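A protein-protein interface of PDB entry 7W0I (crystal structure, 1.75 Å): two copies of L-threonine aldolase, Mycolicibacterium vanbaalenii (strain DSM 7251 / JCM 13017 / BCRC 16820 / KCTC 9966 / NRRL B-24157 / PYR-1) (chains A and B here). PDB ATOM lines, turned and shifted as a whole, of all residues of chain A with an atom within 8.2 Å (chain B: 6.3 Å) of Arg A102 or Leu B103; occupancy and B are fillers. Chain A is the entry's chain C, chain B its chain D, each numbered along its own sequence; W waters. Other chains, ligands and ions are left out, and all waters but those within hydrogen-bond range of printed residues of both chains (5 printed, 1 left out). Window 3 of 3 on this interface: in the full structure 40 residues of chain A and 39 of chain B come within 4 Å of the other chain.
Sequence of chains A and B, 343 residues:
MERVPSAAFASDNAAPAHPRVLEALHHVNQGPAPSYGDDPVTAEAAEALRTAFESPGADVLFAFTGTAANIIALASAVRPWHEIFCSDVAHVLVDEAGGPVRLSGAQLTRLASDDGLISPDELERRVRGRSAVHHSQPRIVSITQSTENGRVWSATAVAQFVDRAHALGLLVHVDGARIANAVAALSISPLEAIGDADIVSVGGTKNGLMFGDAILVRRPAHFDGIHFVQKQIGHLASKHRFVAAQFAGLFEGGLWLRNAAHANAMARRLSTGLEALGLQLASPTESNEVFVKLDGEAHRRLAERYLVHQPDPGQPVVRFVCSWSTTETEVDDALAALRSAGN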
ATOM      1  N   ILE A  71      -9.969 -16.255  -4.728  1.00  0.00           N
ATOM      2  CA  ILE A  71      -8.792 -16.348  -3.869  1.00  0.00           C
ATOM      3  C   ILE A  71      -7.531 -16.019  -4.651  1.00  0.00           C
ATOM      4  O   ILE A  71      -6.661 -15.283  -4.167  1.00  0.00           O
ATOM      5  CB  ILE A  71      -8.705 -17.750  -3.239  1.00  0.00           C
ATOM      6  CG1 ILE A  71      -9.797 -17.936  -2.188  1.00  0.00           C
ATOM      7  CG2 ILE A  71      -7.319 -17.997  -2.672  1.00  0.00           C
ATOM      8  CD1 ILE A  71      -9.983 -19.410  -1.814  1.00  0.00           C
ATOM      9  N   ALA A  75      -5.487 -12.780  -3.508  1.00  0.00           N
ATOM     10  CA  ALA A  75      -4.208 -13.077  -2.879  1.00  0.00           C
ATOM     11  C   ALA A  75      -3.038 -12.597  -3.725  1.00  0.00           C
ATOM     12  O   ALA A  75      -2.014 -12.177  -3.172  1.00  0.00           O
ATOM     13  CB  ALA A  75      -4.105 -14.582  -2.593  1.00  0.00           C
ATOM     14  N   PRO A  80       0.470  -9.486   3.124  1.00  0.00           N
ATOM     15  CA  PRO A  80      -0.337  -9.714   4.337  1.00  0.00           C
ATOM     16  C   PRO A  80      -0.675  -8.460   5.120  1.00  0.00           C
ATOM     17  O   PRO A  80      -1.700  -8.436   5.812  1.00  0.00           O
ATOM     18  CB  PRO A  80       0.546 -10.663   5.158  1.00  0.00           C
ATOM     19  CG  PRO A  80       1.262 -11.447   4.093  1.00  0.00           C
ATOM     20  CD  PRO A  80       1.645 -10.375   3.094  1.00  0.00           C
ATOM     21  N   ILE A  84      -8.082  -5.754   2.327  1.00  0.00           N
ATOM     22  CA  ILE A  84      -9.073  -6.020   1.281  1.00  0.00           C
ATOM     23  C   ILE A  84     -10.437  -5.544   1.778  1.00  0.00           C
ATOM     24  O   ILE A  84     -10.774  -5.728   2.956  1.00  0.00           O
ATOM     25  CB  ILE A  84      -9.118  -7.522   0.919  1.00  0.00           C
ATOM     26  CG1 ILE A  84      -7.713  -8.073   0.619  1.00  0.00           C
ATOM     27  CG2 ILE A  84     -10.092  -7.793  -0.247  1.00  0.00           C
ATOM     28  CD1 ILE A  84      -7.656  -9.615   0.692  1.00  0.00           C
ATOM     29  N   GLU A  96     -16.892 -18.638   1.595  1.00  0.00           N
ATOM     30  CA  GLU A  96     -15.666 -19.299   1.171  1.00  0.00           C
ATOM     31  C   GLU A  96     -14.866 -19.816   2.360  1.00  0.00           C
ATOM     32  O   GLU A  96     -13.666 -20.101   2.228  1.00  0.00           O
ATOM     33  CB  GLU A  96     -14.833 -18.350   0.299  1.00  0.00           C
ATOM     34  CG  GLU A  96     -15.569 -18.036  -1.010  1.00  0.00           C
ATOM     35  CD  GLU A  96     -14.852 -17.071  -1.930  1.00  0.00           C
ATOM     36  OE1 GLU A  96     -13.640 -16.873  -1.765  1.00  0.00           O
ATOM     37  OE2 GLU A  96     -15.524 -16.522  -2.836  1.00  0.00           O
ATOM     38  N   ALA A  97     -15.517 -19.956   3.519  1.00  0.00           N
ATOM     39  CA  ALA A  97     -14.871 -20.395   4.756  1.00  0.00           C
ATOM     40  C   ALA A  97     -13.591 -19.599   5.043  1.00  0.00           C
ATOM     41  O   ALA A  97     -12.656 -20.109   5.659  1.00  0.00           O
ATOM     42  CB  ALA A  97     -14.589 -21.905   4.728  1.00  0.00           C
ATOM     43  N   GLY A  98     -13.568 -18.333   4.637  1.00  0.00           N
ATOM     44  CA  GLY A  98     -12.413 -17.491   4.913  1.00  0.00           C
ATOM     45  C   GLY A  98     -11.203 -17.750   4.046  1.00  0.00           C
ATOM     46  O   GLY A  98     -10.119 -17.236   4.356  1.00  0.00           O
ATOM     47  N   GLY A  99     -11.363 -18.490   2.945  1.00  0.00           N
ATOM     48  CA  GLY A  99     -10.279 -18.786   2.029  1.00  0.00           C
ATOM     49  C   GLY A  99      -9.441 -17.581   1.612  1.00  0.00           C
ATOM     50  O   GLY A  99      -8.205 -17.620   1.640  1.00  0.00           O
ATOM     51  N   PRO A 100     -10.097 -16.489   1.191  1.00  0.00           N
ATOM     52  CA  PRO A 100      -9.323 -15.295   0.781  1.00  0.00           C
ATOM     53  C   PRO A 100      -8.436 -14.747   1.882  1.00  0.00           C
ATOM     54  O   PRO A 100      -7.286 -14.355   1.629  1.00  0.00           O
ATOM     55  CB  PRO A 100     -10.416 -14.299   0.386  1.00  0.00           C
ATOM     56  CG  PRO A 100     -11.553 -15.151  -0.065  1.00  0.00           C
ATOM     57  CD  PRO A 100     -11.530 -16.366   0.842  1.00  0.00           C
ATOM     58  N   VAL A 101      -8.952 -14.700   3.108  1.00  0.00           N
ATOM     59  CA  VAL A 101      -8.155 -14.243   4.245  1.00  0.00           C
ATOM     60  C   VAL A 101      -7.012 -15.215   4.546  1.00  0.00           C
ATOM     61  O   VAL A 101      -5.874 -14.799   4.824  1.00  0.00           O
ATOM     62  CB  VAL A 101      -9.087 -14.043   5.452  1.00  0.00           C
ATOM     63  CG1 VAL A 101      -8.276 -13.920   6.757  1.00  0.00           C
ATOM     64  CG2 VAL A 101      -9.931 -12.793   5.232  1.00  0.00           C
ATOM     65  N   ARG A 102      -7.291 -16.518   4.518  1.00  0.00           N
ATOM     66  CA  ARG A 102      -6.251 -17.499   4.829  1.00  0.00           C
ATOM     67  C   ARG A 102      -5.097 -17.428   3.837  1.00  0.00           C
ATOM     68  O   ARG A 102      -3.923 -17.435   4.239  1.00  0.00           O
ATOM     69  CB  ARG A 102      -6.833 -18.925   4.846  1.00  0.00           C
ATOM     70  CG  ARG A 102      -5.746 -19.973   5.146  1.00  0.00           C
ATOM     71  CD  ARG A 102      -6.250 -21.407   5.194  1.00  0.00           C
ATOM     72  NE  ARG A 102      -5.156 -22.303   5.575  1.00  0.00           N
ATOM     73  CZ  ARG A 102      -5.302 -23.506   6.124  1.00  0.00           C
ATOM     74  NH1 ARG A 102      -6.515 -23.999   6.373  1.00  0.00           N
ATOM     75  NH2 ARG A 102      -4.220 -24.219   6.430  1.00  0.00           N
ATOM     76  N   LEU A 103      -5.402 -17.332   2.544  1.00  0.00           N
ATOM     77  CA  LEU A 103      -4.321 -17.377   1.576  1.00  0.00           C
ATOM     78  C   LEU A 103      -3.615 -16.025   1.487  1.00  0.00           C
ATOM     79  O   LEU A 103      -2.382 -15.981   1.377  1.00  0.00           O
ATOM     80  CB  LEU A 103      -4.834 -17.802   0.206  1.00  0.00           C
ATOM     81  CG  LEU A 103      -3.651 -18.272  -0.668  1.00  0.00           C
ATOM     82  CD1 LEU A 103      -3.101 -19.593  -0.146  1.00  0.00           C
ATOM     83  CD2 LEU A 103      -3.986 -18.379  -2.151  1.00  0.00           C
ATOM     84  N   SER A 104      -4.372 -14.911   1.517  1.00  0.00           N
ATOM     85  CA  SER A 104      -3.730 -13.589   1.410  1.00  0.00           C
ATOM     86  C   SER A 104      -2.945 -13.199   2.665  1.00  0.00           C
ATOM     87  O   SER A 104      -2.012 -12.390   2.583  1.00  0.00           O
ATOM     88  CB  SER A 104      -4.763 -12.512   1.092  1.00  0.00           C
ATOM     89  OG  SER A 104      -5.652 -12.309   2.170  1.00  0.00           O
ATOM     90  N   GLY A 105      -3.358 -13.672   3.834  1.00  0.00           N
ATOM     91  CA  GLY A 105      -2.824 -13.179   5.093  1.00  0.00           C
ATOM     92  C   GLY A 105      -3.344 -11.827   5.539  1.00  0.00           C
ATOM     93  O   GLY A 105      -2.954 -11.370   6.622  1.00  0.00           O
ATOM     94  N   ALA A 106      -4.252 -11.209   4.774  1.00  0.00           N
ATOM     95  CA  ALA A 106      -4.726  -9.838   4.933  1.00  0.00           C
ATOM     96  C   ALA A 106      -6.124  -9.779   5.530  1.00  0.00           C
ATOM     97  O   ALA A 106      -6.938 -10.683   5.330  1.00  0.00           O
ATOM     98  CB  ALA A 106      -4.762  -9.130   3.571  1.00  0.00           C
ATOM     99  N   GLN A 107      -6.408  -8.682   6.240  1.00  0.00           N
ATOM    100  CA  GLN A 107      -7.755  -8.469   6.754  1.00  0.00           C
ATOM    101  C   GLN A 107      -8.738  -8.219   5.614  1.00  0.00           C
ATOM    102  O   GLN A 107      -8.414  -7.542   4.628  1.00  0.00           O
ATOM    103  CB  GLN A 107      -7.770  -7.292   7.729  1.00  0.00           C
ATOM    104  CG  GLN A 107      -6.888  -7.527   8.981  1.00  0.00           C
ATOM    105  CD  GLN A 107      -7.328  -6.715  10.186  1.00  0.00           C
ATOM    106  OE1 GLN A 107      -8.230  -7.121  10.934  1.00  0.00           O
ATOM    107  NE2 GLN A 107      -6.713  -5.542  10.366  1.00  0.00           N
ATOM    108  N   LEU A 108      -9.950  -8.773   5.748  1.00  0.00           N
ATOM    109  CA  LEU A 108     -11.049  -8.541   4.802  1.00  0.00           C
ATOM    110  C   LEU A 108     -12.127  -7.715   5.500  1.00  0.00           C
ATOM    111  O   LEU A 108     -12.847  -8.224   6.367  1.00  0.00           O
ATOM    112  CB  LEU A 108     -11.615  -9.864   4.281  1.00  0.00           C
ATOM    113  CG  LEU A 108     -12.797  -9.750   3.308  1.00  0.00           C
ATOM    114  CD1 LEU A 108     -12.367  -9.020   2.053  1.00  0.00           C
ATOM    115  CD2 LEU A 108     -13.348 -11.142   2.954  1.00  0.00           C
ATOM    116  N   GLN A 232       0.143 -22.981  -6.538  1.00  0.00           N
ATOM    117  CA  GLN A 232       0.329 -23.335  -5.135  1.00  0.00           C
ATOM    118  C   GLN A 232      -0.942 -23.841  -4.476  1.00  0.00           C
ATOM    119  O   GLN A 232      -0.852 -24.553  -3.474  1.00  0.00           O
ATOM    120  CB  GLN A 232       0.854 -22.132  -4.344  1.00  0.00           C
ATOM    121  CG  GLN A 232       2.349 -21.896  -4.499  1.00  0.00           C
ATOM    122  CD  GLN A 232       2.865 -20.843  -3.531  1.00  0.00           C
ATOM    123  OE1 GLN A 232       2.324 -19.744  -3.453  1.00  0.00           O
ATOM    124  NE2 GLN A 232       3.903 -21.189  -2.771  1.00  0.00           N
ATOM    125  N   ILE A 233      -2.117 -23.488  -4.986  1.00  0.00           N
ATOM    126  CA  ILE A 233      -3.339 -24.024  -4.402  1.00  0.00           C
ATOM    127  C   ILE A 233      -3.960 -25.096  -5.298  1.00  0.00           C
ATOM    128  O   ILE A 233      -5.133 -25.429  -5.145  1.00  0.00           O
ATOM    129  CB  ILE A 233      -4.350 -22.920  -4.044  1.00  0.00           C
ATOM    130  CG1 ILE A 233      -4.746 -22.080  -5.258  1.00  0.00           C
ATOM    131  CG2 ILE A 233      -3.797 -22.051  -2.912  1.00  0.00           C
ATOM    132  CD1 ILE A 233      -6.115 -21.406  -5.071  1.00  0.00           C
ATOM    133  N   ILE B  71      -1.882 -31.339  -1.015  1.00  0.00           N
ATOM    134  CA  ILE B  71      -1.903 -30.174  -0.135  1.00  0.00           C
ATOM    135  C   ILE B  71      -2.978 -30.332   0.928  1.00  0.00           C
ATOM    136  O   ILE B  71      -2.742 -30.069   2.113  1.00  0.00           O
ATOM    137  CB  ILE B  71      -2.103 -28.890  -0.958  1.00  0.00           C
ATOM    138  CG1 ILE B  71      -0.849 -28.571  -1.755  1.00  0.00           C
ATOM    139  CG2 ILE B  71      -2.363 -27.732  -0.077  1.00  0.00           C
ATOM    140  CD1 ILE B  71      -1.114 -27.504  -2.785  1.00  0.00           C
ATOM    141  N   ILE B  72      -4.173 -30.777   0.520  1.00  0.00           N
ATOM    142  CA  ILE B  72      -5.280 -30.949   1.465  1.00  0.00           C
ATOM    143  C   ILE B  72      -4.959 -32.030   2.494  1.00  0.00           C
ATOM    144  O   ILE B  72      -5.183 -31.844   3.703  1.00  0.00           O
ATOM    145  CB  ILE B  72      -6.585 -31.247   0.703  1.00  0.00           C
ATOM    146  CG1 ILE B  72      -7.024 -30.022  -0.103  1.00  0.00           C
ATOM    147  CG2 ILE B  72      -7.709 -31.650   1.679  1.00  0.00           C
ATOM    148  CD1 ILE B  72      -8.065 -30.339  -1.163  1.00  0.00           C
ATOM    149  N   ALA B  75      -1.875 -30.601   4.795  1.00  0.00           N
ATOM    150  CA  ALA B  75      -2.229 -29.456   5.617  1.00  0.00           C
ATOM    151  C   ALA B  75      -3.271 -29.830   6.656  1.00  0.00           C
ATOM    152  O   ALA B  75      -3.256 -29.282   7.764  1.00  0.00           O
ATOM    153  CB  ALA B  75      -2.728 -28.305   4.745  1.00  0.00           C
ATOM    154  N   SER B  76      -4.180 -30.755   6.335  1.00  0.00           N
ATOM    155  CA  SER B  76      -5.122 -31.165   7.366  1.00  0.00           C
ATOM    156  C   SER B  76      -4.461 -32.028   8.438  1.00  0.00           C
ATOM    157  O   SER B  76      -5.023 -32.179   9.528  1.00  0.00           O
ATOM    158  CB  SER B  76      -6.316 -31.902   6.721  1.00  0.00           C
ATOM    159  OG  SER B  76      -5.961 -33.238   6.361  1.00  0.00           O
ATOM    160  N   GLY B  98       5.887 -25.344  -3.707  1.00  0.00           N
ATOM    161  CA  GLY B  98       5.846 -25.187  -2.262  1.00  0.00           C
ATOM    162  C   GLY B  98       4.467 -25.080  -1.665  1.00  0.00           C
ATOM    163  O   GLY B  98       4.343 -24.648  -0.516  1.00  0.00           O
ATOM    164  N   GLY B  99       3.426 -25.444  -2.421  1.00  0.00           N
ATOM    165  CA  GLY B  99       2.056 -25.401  -1.962  1.00  0.00           C
ATOM    166  C   GLY B  99       1.823 -26.044  -0.604  1.00  0.00           C
ATOM    167  O   GLY B  99       1.176 -25.452   0.260  1.00  0.00           O
ATOM    168  N   PRO B 100       2.320 -27.275  -0.390  1.00  0.00           N
ATOM    169  CA  PRO B 100       2.124 -27.917   0.931  1.00  0.00           C
ATOM    170  C   PRO B 100       2.677 -27.097   2.088  1.00  0.00           C
ATOM    171  O   PRO B 100       2.033 -26.971   3.144  1.00  0.00           O
ATOM    172  CB  PRO B 100       2.882 -29.241   0.784  1.00  0.00           C
ATOM    173  CG  PRO B 100       2.766 -29.568  -0.688  1.00  0.00           C
ATOM    174  CD  PRO B 100       2.850 -28.227  -1.391  1.00  0.00           C
ATOM    175  N   VAL B 101       3.869 -26.537   1.902  1.00  0.00           N
ATOM    176  CA  VAL B 101       4.467 -25.684   2.926  1.00  0.00           C
ATOM    177  C   VAL B 101       3.650 -24.413   3.121  1.00  0.00           C
ATOM    178  O   VAL B 101       3.388 -23.998   4.257  1.00  0.00           O
ATOM    179  CB  VAL B 101       5.924 -25.365   2.550  1.00  0.00           C
ATOM    180  CG1 VAL B 101       6.450 -24.138   3.349  1.00  0.00           C
ATOM    181  CG2 VAL B 101       6.791 -26.596   2.757  1.00  0.00           C
ATOM    182  N   ARG B 102       3.224 -23.779   2.028  1.00  0.00           N
ATOM    183  CA  ARG B 102       2.469 -22.539   2.173  1.00  0.00           C
ATOM    184  C   ARG B 102       1.158 -22.781   2.926  1.00  0.00           C
ATOM    185  O   ARG B 102       0.821 -22.015   3.840  1.00  0.00           O
ATOM    186  CB  ARG B 102       2.180 -21.906   0.816  1.00  0.00           C
ATOM    187  CG  ARG B 102       1.374 -20.597   0.957  1.00  0.00           C
ATOM    188  CD  ARG B 102       1.021 -19.928  -0.383  1.00  0.00           C
ATOM    189  NE  ARG B 102       0.318 -18.673  -0.126  1.00  0.00           N
ATOM    190  CZ  ARG B 102       0.264 -17.633  -0.955  1.00  0.00           C
ATOM    191  NH1 ARG B 102       0.880 -17.662  -2.128  1.00  0.00           N
ATOM    192  NH2 ARG B 102      -0.404 -16.547  -0.592  1.00  0.00           N
ATOM    193  N   LEU B 103       0.415 -23.859   2.592  1.00  0.00           N
ATOM    194  CA  LEU B 103      -0.869 -24.056   3.279  1.00  0.00           C
ATOM    195  C   LEU B 103      -0.708 -24.509   4.708  1.00  0.00           C
ATOM    196  O   LEU B 103      -1.433 -24.027   5.584  1.00  0.00           O
ATOM    197  CB  LEU B 103      -1.742 -25.183   2.731  1.00  0.00           C
ATOM    198  CG  LEU B 103      -3.278 -24.945   2.600  1.00  0.00           C
ATOM    199  CD1 LEU B 103      -3.728 -23.529   2.265  1.00  0.00           C
ATOM    200  CD2 LEU B 103      -4.272 -26.065   2.235  1.00  0.00           C
ATOM    201  N   SER B 104       0.161 -25.505   4.945  1.00  0.00           N
ATOM    202  CA  SER B 104       0.307 -26.068   6.285  1.00  0.00           C
ATOM    203  C   SER B 104       0.978 -25.097   7.241  1.00  0.00           C
ATOM    204  O   SER B 104       0.753 -25.187   8.452  1.00  0.00           O
ATOM    205  CB  SER B 104       1.097 -27.376   6.228  1.00  0.00           C
ATOM    206  OG  SER B 104       2.427 -27.113   5.829  1.00  0.00           O
ATOM    207  N   GLY B 105       1.848 -24.229   6.729  1.00  0.00           N
ATOM    208  CA  GLY B 105       2.697 -23.408   7.567  1.00  0.00           C
ATOM    209  C   GLY B 105       3.878 -24.132   8.176  1.00  0.00           C
ATOM    210  O   GLY B 105       4.590 -23.533   8.996  1.00  0.00           O
ATOM    211  N   ALA B 106       4.076 -25.410   7.833  1.00  0.00           N
ATOM    212  CA  ALA B 106       5.044 -26.312   8.456  1.00  0.00           C
ATOM    213  C   ALA B 106       6.237 -26.584   7.549  1.00  0.00           C
ATOM    214  O   ALA B 106       6.123 -26.536   6.320  1.00  0.00           O
ATOM    215  CB  ALA B 106       4.375 -27.644   8.819  1.00  0.00           C
ATOM    216  N   PHE B 228     -12.954 -28.466   5.648  1.00  0.00           N
ATOM    217  CA  PHE B 228     -12.770 -27.016   5.614  1.00  0.00           C
ATOM    218  C   PHE B 228     -11.539 -26.631   4.800  1.00  0.00           C
ATOM    219  O   PHE B 228     -11.553 -25.615   4.087  1.00  0.00           O
ATOM    220  CB  PHE B 228     -12.658 -26.441   7.033  1.00  0.00           C
ATOM    221  CG  PHE B 228     -13.959 -26.412   7.769  1.00  0.00           C
ATOM    222  CD1 PHE B 228     -14.958 -25.512   7.405  1.00  0.00           C
ATOM    223  CD2 PHE B 228     -14.203 -27.299   8.802  1.00  0.00           C
ATOM    224  CE1 PHE B 228     -16.176 -25.496   8.065  1.00  0.00           C
ATOM    225  CE2 PHE B 228     -15.439 -27.298   9.467  1.00  0.00           C
ATOM    226  CZ  PHE B 228     -16.418 -26.411   9.094  1.00  0.00           C
ATOM    227  N   VAL B 229     -10.452 -27.400   4.920  1.00  0.00           N
ATOM    228  CA  VAL B 229      -9.252 -27.106   4.134  1.00  0.00           C
ATOM    229  C   VAL B 229      -9.569 -27.217   2.654  1.00  0.00           C
ATOM    230  O   VAL B 229      -9.208 -26.346   1.855  1.00  0.00           O
ATOM    231  CB  VAL B 229      -8.097 -28.047   4.530  1.00  0.00           C
ATOM    232  CG1 VAL B 229      -6.839 -27.782   3.662  1.00  0.00           C
ATOM    233  CG2 VAL B 229      -7.753 -27.882   6.011  1.00  0.00           C
ATOM    234  N   GLN B 232     -11.511 -24.158   1.608  1.00  0.00           N
ATOM    235  CA  GLN B 232     -10.739 -22.923   1.682  1.00  0.00           C
ATOM    236  C   GLN B 232      -9.787 -22.741   0.512  1.00  0.00           C
ATOM    237  O   GLN B 232      -9.352 -21.609   0.273  1.00  0.00           O
ATOM    238  CB  GLN B 232      -9.942 -22.869   2.986  1.00  0.00           C
ATOM    239  CG  GLN B 232     -10.757 -22.493   4.220  1.00  0.00           C
ATOM    240  CD  GLN B 232      -9.853 -22.213   5.430  1.00  0.00           C
ATOM    241  OE1 GLN B 232      -9.039 -23.050   5.817  1.00  0.00           O
ATOM    242  NE2 GLN B 232      -9.994 -21.034   6.020  1.00  0.00           N
ATOM    243  N   ILE B 233      -9.389 -23.802  -0.182  1.00  0.00           N
ATOM    244  CA  ILE B 233      -8.532 -23.603  -1.348  1.00  0.00           C
ATOM    245  C   ILE B 233      -9.311 -23.812  -2.641  1.00  0.00           C
ATOM    246  O   ILE B 233      -8.710 -23.976  -3.708  1.00  0.00           O
ATOM    247  CB  ILE B 233      -7.256 -24.462  -1.306  1.00  0.00           C
ATOM    248  CG1 ILE B 233      -7.557 -25.958  -1.201  1.00  0.00           C
ATOM    249  CG2 ILE B 233      -6.304 -23.938  -0.194  1.00  0.00           C
ATOM    250  CD1 ILE B 233      -6.362 -26.823  -1.632  1.00  0.00           C
HETATM  251  O   HOH W   1      -9.799 -17.838   7.010  1.00  0.00           O
HETATM  252  O   HOH W   2       5.806 -22.421  -0.233  1.00  0.00           O
HETATM  253  O   HOH W   3      -0.719 -23.657  -0.845  1.00  0.00           O
HETATM  254  O   HOH W   4      -2.510 -21.212   5.670  1.00  0.00           O
HETATM  255  O   HOH W   5      -0.547 -18.067   2.563  1.00  0.00           O
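O of Ala A97 sits at hydrogen-bond distance from NE2 of Gln B232 (2.8 Å).
The backbone carbonyl oxygen of Leu B103 lies within hydrogen-bond range of the guanidinium group of Arg A102, at 2.9 Å.
The side-chain amide oxygen of Gln B232 sits at hydrogen-bond distance from the guanidinium group of Arg A102 (2.8 Å).
NH2 of Arg B102 is in hydrogen-bond range of O of Leu A103.
The side-chain amide oxygen of Gln A232 lies within hydrogen-bond range of the guanidinium group of Arg B102 (2.9 Å).
Among the printed residues, merely in contact across the chains: Gln A232 with Ile B71, Ile A71 with Gln B232, Gln A232 with Gly B99, Gly A99 with Gln B232 and Ile A233 with Ile B233.
Printed residues of chain B within 4 Å of Ile A71: Gln B232 (3.1 Å).
Val A101 touches none of the printed residues of chain B.
Printed residues of chain B within 4 Å of Leu A103: Arg B102 (2.8 Å).
Of the printed residues of chain B, Ile A233 touches Ile B233 (3.9 Å).
Of the printed residues of chain A, Ile B71 touches Gln A232 (3.0 Å).
Leu B103 touches one residue of chain A.
Phe B228 touches none of the printed residues of chain A.
Of the printed residues of chain A, Ile B233 touches Ile A233 (3.9 Å).
The nearest residue of chain B that does not touch Arg A102 is Val B229 (4.1 Å).
The nearest printed residue of chain B that does not touch Ile A71 is Ile B233 (4.5 Å).
Printed residues of chain A that touch a printed residue of chain B: Ile A71, Ala A97, Gly A99, Arg A102, Leu A103, Gln A232 and Ile A233.
Hydrophobic or aromatic side chains of chain A that line the printed part of chain B: Ile A71, Ala A97, Leu A103 and Ile A233.
Along chain A the printed residues that touch a printed residue of chain B span positions 71 to 233.
Of the 17 printed residues of chain B, 6 touch a printed residue of chain A.
Among the printed residues, 10 pairs touch across the chains.
Among the printed residues, no Asp or Glu carboxylate lies within 4 Å of a Lys or Arg side-chain nitrogen of the other chain.
Ile A71 touches Gln B232, and with the chains exchanged Gln A232 touches Ile B71.
Gly A99 touches Gln B232, and with the chains exchanged Gln A232 touches Gly B99.
Arg A102 touches Leu B103, and with the chains exchanged Leu A103 touches Arg B102.
Ile B233 touches its own counterpart, Ile A233.
13 positions are printed for both chains.
Of the 10 pairs that touch across the chains among the printed residues, 9 have their exchanged pair printed and touching as well.
Water W2 bridges the backbone carbonyl oxygen of Gly B98 (2.7 Å) and the side-chain amide nitrogen of Gln A232 (3.4 Å).
Water W1 bridges the backbone carbonyl oxygen of Gly A98 (2.7 Å) and the side-chain amide nitrogen of Gln B232 (3.4 Å).
Water W3 bridges O of Gln A232 (2.8 Å) and O of Gly B99 (2.8 Å).
Water W4 bridges the guanidinium group (NE) of Arg A102 (2.9 Å) and the backbone carbonyl oxygen (O) of Leu B103 (3.0 Å).
Water W5 bridges the guanidinium group of Arg B102 and the backbone carbonyl oxygen of Leu A103.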
